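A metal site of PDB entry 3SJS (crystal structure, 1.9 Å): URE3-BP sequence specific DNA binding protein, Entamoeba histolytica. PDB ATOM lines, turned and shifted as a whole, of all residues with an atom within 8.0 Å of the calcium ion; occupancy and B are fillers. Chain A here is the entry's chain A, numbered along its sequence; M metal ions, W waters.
Water W1 lies within hydrogen-bond range of the side-chain carboxylate of Glu 108 (2.9 Å) and the backbone NH of Ser 105 (3.4 Å).
The calcium ion is bound by the side-chain carboxylate of Asp 97 (2.2 Å), the side-chain carboxylate of Asp 99 (2.3 Å), the backbone carbonyl oxygen of His 103 (2.4 Å), water W1 (2.4 Å) and the side-chain amide oxygen of Asn 101 (2.5 Å).
The calcium ion has five donor atoms within binding distance.
Merely in contact with the calcium ion: Glu 108 (3.4 Å).
Along chain A the residues within 4 Å of the calcium ion span positions 97 to 108.
OD1 of Asp 97 lies close to N of Phe 100.
N of Gly 102 lies within hydrogen-bond range of OD2 of Asp 97, 2.8 Å away.
OE2 of Glu 108 sits at hydrogen-bond distance from OG1 of Thr 98 (2.7 Å).
The side-chain carboxylate (OE1) of Glu 108 lies within hydrogen-bond range of the backbone NH (N) of Ser 105 (2.9 Å).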
ATOM      1  N   SER A  32      22.248  18.561 -33.428  1.00  0.00           N
ATOM      2  CA  SER A  32      21.097  17.674 -33.181  1.00  0.00           C
ATOM      3  C   SER A  32      19.758  18.406 -33.152  1.00  0.00           C
ATOM      4  O   SER A  32      18.757  17.828 -33.531  1.00  0.00           O
ATOM      5  CB  SER A  32      21.223  16.861 -31.885  1.00  0.00           C
ATOM      6  OG  SER A  32      21.361  17.659 -30.727  1.00  0.00           O
ATOM      7  N   VAL A  33      19.748  19.659 -32.707  1.00  0.00           N
ATOM      8  CA  VAL A  33      18.522  20.443 -32.623  1.00  0.00           C
ATOM      9  C   VAL A  33      18.166  20.966 -33.988  1.00  0.00           C
ATOM     10  O   VAL A  33      17.012  20.884 -34.387  1.00  0.00           O
ATOM     11  CB  VAL A  33      18.639  21.599 -31.561  1.00  0.00           C
ATOM     12  CG1 VAL A  33      17.428  22.495 -31.590  1.00  0.00           C
ATOM     13  CG2 VAL A  33      18.788  21.034 -30.138  1.00  0.00           C
ATOM     14  N   THR A  67      18.584  22.332 -17.398  1.00  0.00           N
ATOM     15  CA  THR A  67      18.114  21.284 -18.240  1.00  0.00           C
ATOM     16  C   THR A  67      16.994  20.577 -17.464  1.00  0.00           C
ATOM     17  O   THR A  67      16.885  20.698 -16.246  1.00  0.00           O
ATOM     18  CB  THR A  67      19.202  20.284 -18.561  1.00  0.00           C
ATOM     19  OG1 THR A  67      19.619  19.670 -17.359  1.00  0.00           O
ATOM     20  CG2 THR A  67      20.395  20.964 -19.235  1.00  0.00           C
ATOM     21  N   LEU A  68      16.150  19.862 -18.179  1.00  0.00           N
ATOM     22  CA  LEU A  68      15.076  19.141 -17.552  1.00  0.00           C
ATOM     23  C   LEU A  68      15.276  17.668 -17.795  1.00  0.00           C
ATOM     24  O   LEU A  68      15.616  17.226 -18.895  1.00  0.00           O
ATOM     25  CB  LEU A  68      13.721  19.585 -18.059  1.00  0.00           C
ATOM     26  CG  LEU A  68      13.320  21.057 -17.907  1.00  0.00           C
ATOM     27  CD1 LEU A  68      11.982  21.260 -18.552  1.00  0.00           C
ATOM     28  CD2 LEU A  68      13.329  21.460 -16.430  1.00  0.00           C
ATOM     29  N   MET A  93      10.466  13.075 -23.889  1.00  0.00           N
ATOM     30  CA  MET A  93      11.928  12.898 -23.936  1.00  0.00           C
ATOM     31  C   MET A  93      12.343  12.312 -25.278  1.00  0.00           C
ATOM     32  O   MET A  93      13.370  12.707 -25.840  1.00  0.00           O
ATOM     33  CB  MET A  93      12.456  11.982 -22.821  1.00  0.00           C
ATOM     34  CG  MET A  93      12.301  12.498 -21.400  1.00  0.00           C
ATOM     35  SD  MET A  93      13.086  14.121 -21.051  1.00  0.00           S
ATOM     36  CE  MET A  93      14.733  13.704 -21.490  1.00  0.00           C
ATOM     37  N   PHE A  96      12.099  15.158 -27.932  1.00  0.00           N
ATOM     38  CA  PHE A  96      12.814  16.430 -27.770  1.00  0.00           C
ATOM     39  C   PHE A  96      14.257  16.373 -27.266  1.00  0.00           C
ATOM     40  O   PHE A  96      15.015  17.323 -27.468  1.00  0.00           O
ATOM     41  CB  PHE A  96      11.973  17.398 -26.942  1.00  0.00           C
ATOM     42  CG  PHE A  96      10.689  17.805 -27.644  1.00  0.00           C
ATOM     43  CD1 PHE A  96      10.719  18.694 -28.714  1.00  0.00           C
ATOM     44  CD2 PHE A  96       9.485  17.248 -27.298  1.00  0.00           C
ATOM     45  CE1 PHE A  96       9.545  19.022 -29.371  1.00  0.00           C
ATOM     46  CE2 PHE A  96       8.327  17.588 -27.944  1.00  0.00           C
ATOM     47  CZ  PHE A  96       8.358  18.464 -28.970  1.00  0.00           C
ATOM     48  N   ASP A  97      14.641  15.259 -26.638  1.00  0.00           N
ATOM     49  CA  ASP A  97      16.036  14.981 -26.258  1.00  0.00           C
ATOM     50  C   ASP A  97      16.765  14.462 -27.499  1.00  0.00           C
ATOM     51  O   ASP A  97      16.977  13.281 -27.694  1.00  0.00           O
ATOM     52  CB  ASP A  97      16.085  13.996 -25.105  1.00  0.00           C
ATOM     53  CG  ASP A  97      17.488  13.585 -24.694  1.00  0.00           C
ATOM     54  OD1 ASP A  97      18.467  14.291 -25.009  1.00  0.00           O
ATOM     55  OD2 ASP A  97      17.618  12.546 -24.050  1.00  0.00           O
ATOM     56  N   THR A  98      17.185  15.399 -28.328  1.00  0.00           N
ATOM     57  CA  THR A  98      17.702  15.120 -29.666  1.00  0.00           C
ATOM     58  C   THR A  98      19.112  14.527 -29.662  1.00  0.00           C
ATOM     59  O   THR A  98      19.534  13.970 -30.680  1.00  0.00           O
ATOM     60  CB  THR A  98      17.715  16.428 -30.526  1.00  0.00           C
ATOM     61  OG1 THR A  98      18.677  17.333 -29.985  1.00  0.00           O
ATOM     62  CG2 THR A  98      16.406  17.114 -30.500  1.00  0.00           C
ATOM     63  N   ASP A  99      19.841  14.641 -28.548  1.00  0.00           N
ATOM     64  CA  ASP A  99      21.168  14.009 -28.445  1.00  0.00           C
ATOM     65  C   ASP A  99      21.189  12.832 -27.503  1.00  0.00           C
ATOM     66  O   ASP A  99      22.258  12.328 -27.129  1.00  0.00           O
ATOM     67  CB  ASP A  99      22.279  15.000 -28.098  1.00  0.00           C
ATOM     68  CG  ASP A  99      22.082  15.679 -26.777  1.00  0.00           C
ATOM     69  OD1 ASP A  99      20.946  15.655 -26.253  1.00  0.00           O
ATOM     70  OD2 ASP A  99      23.040  16.284 -26.280  1.00  0.00           O
ATOM     71  N   PHE A 100      20.001  12.387 -27.122  1.00  0.00           N
ATOM     72  CA  PHE A 100      19.831  11.157 -26.387  1.00  0.00           C
ATOM     73  C   PHE A 100      20.691  11.117 -25.125  1.00  0.00           C
ATOM     74  O   PHE A 100      21.218  10.065 -24.801  1.00  0.00           O
ATOM     75  CB  PHE A 100      20.191   9.954 -27.268  1.00  0.00           C
ATOM     76  CG  PHE A 100      19.441   9.921 -28.574  1.00  0.00           C
ATOM     77  CD1 PHE A 100      18.101   9.555 -28.610  1.00  0.00           C
ATOM     78  CD2 PHE A 100      20.065  10.283 -29.743  1.00  0.00           C
ATOM     79  CE1 PHE A 100      17.392   9.540 -29.802  1.00  0.00           C
ATOM     80  CE2 PHE A 100      19.361  10.289 -30.929  1.00  0.00           C
ATOM     81  CZ  PHE A 100      18.005   9.909 -30.953  1.00  0.00           C
ATOM     82  N   ASN A 101      20.839  12.231 -24.416  1.00  0.00           N
ATOM     83  CA  ASN A 101      21.619  12.223 -23.180  1.00  0.00           C
ATOM     84  C   ASN A 101      20.774  12.268 -21.907  1.00  0.00           C
ATOM     85  O   ASN A 101      21.336  12.484 -20.841  1.00  0.00           O
ATOM     86  CB  ASN A 101      22.642  13.348 -23.186  1.00  0.00           C
ATOM     87  CG  ASN A 101      22.009  14.708 -23.068  1.00  0.00           C
ATOM     88  OD1 ASN A 101      20.803  14.842 -23.044  1.00  0.00           O
ATOM     89  ND2 ASN A 101      22.841  15.740 -22.994  1.00  0.00           N
ATOM     90  N   GLY A 102      19.465  12.052 -22.008  1.00  0.00           N
ATOM     91  CA  GLY A 102      18.564  12.055 -20.816  1.00  0.00           C
ATOM     92  C   GLY A 102      18.117  13.410 -20.252  1.00  0.00           C
ATOM     93  O   GLY A 102      17.484  13.459 -19.188  1.00  0.00           O
ATOM     94  N   HIS A 103      18.477  14.500 -20.932  1.00  0.00           N
ATOM     95  CA  HIS A 103      18.092  15.855 -20.529  1.00  0.00           C
ATOM     96  C   HIS A 103      17.517  16.598 -21.714  1.00  0.00           C
ATOM     97  O   HIS A 103      17.931  16.381 -22.846  1.00  0.00           O
ATOM     98  CB  HIS A 103      19.296  16.692 -20.110  1.00  0.00           C
ATOM     99  CG  HIS A 103      20.247  15.982 -19.215  1.00  0.00           C
ATOM    100  ND1 HIS A 103      19.852  15.456 -17.997  1.00  0.00           N
ATOM    101  CD2 HIS A 103      21.561  15.709 -19.351  1.00  0.00           C
ATOM    102  CE1 HIS A 103      20.883  14.872 -17.427  1.00  0.00           C
ATOM    103  NE2 HIS A 103      21.938  15.004 -18.227  1.00  0.00           N
ATOM    104  N   ILE A 104      16.586  17.511 -21.438  1.00  0.00           N
ATOM    105  CA  ILE A 104      16.058  18.438 -22.426  1.00  0.00           C
ATOM    106  C   ILE A 104      16.675  19.820 -22.141  1.00  0.00           C
ATOM    107  O   ILE A 104      16.608  20.299 -21.031  1.00  0.00           O
ATOM    108  CB  ILE A 104      14.530  18.441 -22.325  1.00  0.00           C
ATOM    109  CG1 ILE A 104      13.984  17.245 -23.103  1.00  0.00           C
ATOM    110  CG2 ILE A 104      13.938  19.702 -22.868  1.00  0.00           C
ATOM    111  CD1 ILE A 104      12.492  17.064 -22.908  1.00  0.00           C
ATOM    112  N   SER A 105      17.316  20.425 -23.131  1.00  0.00           N
ATOM    113  CA  SER A 105      17.865  21.758 -23.011  1.00  0.00           C
ATOM    114  C   SER A 105      16.747  22.796 -23.006  1.00  0.00           C
ATOM    115  O   SER A 105      15.553  22.484 -23.243  1.00  0.00           O
ATOM    116  CB  SER A 105      18.828  22.055 -24.163  1.00  0.00           C
ATOM    117  OG  SER A 105      18.135  22.116 -25.404  1.00  0.00           O
ATOM    118  N   GLU A 108      15.309  22.776 -26.565  1.00  0.00           N
ATOM    119  CA  GLU A 108      14.424  21.623 -26.751  1.00  0.00           C
ATOM    120  C   GLU A 108      13.101  21.809 -25.976  1.00  0.00           C
ATOM    121  O   GLU A 108      12.019  21.470 -26.465  1.00  0.00           O
ATOM    122  CB  GLU A 108      15.138  20.319 -26.367  1.00  0.00           C
ATOM    123  CG  GLU A 108      16.285  19.998 -27.298  1.00  0.00           C
ATOM    124  CD  GLU A 108      17.280  18.966 -26.765  1.00  0.00           C
ATOM    125  OE1 GLU A 108      17.382  18.762 -25.541  1.00  0.00           O
ATOM    126  OE2 GLU A 108      17.986  18.385 -27.607  1.00  0.00           O
HETATM  127 CA    CA M   1      19.473  16.236 -24.625  1.00  0.00          CA
HETATM  128  O   HOH W   1      19.957  18.564 -24.251  1.00  0.00           O
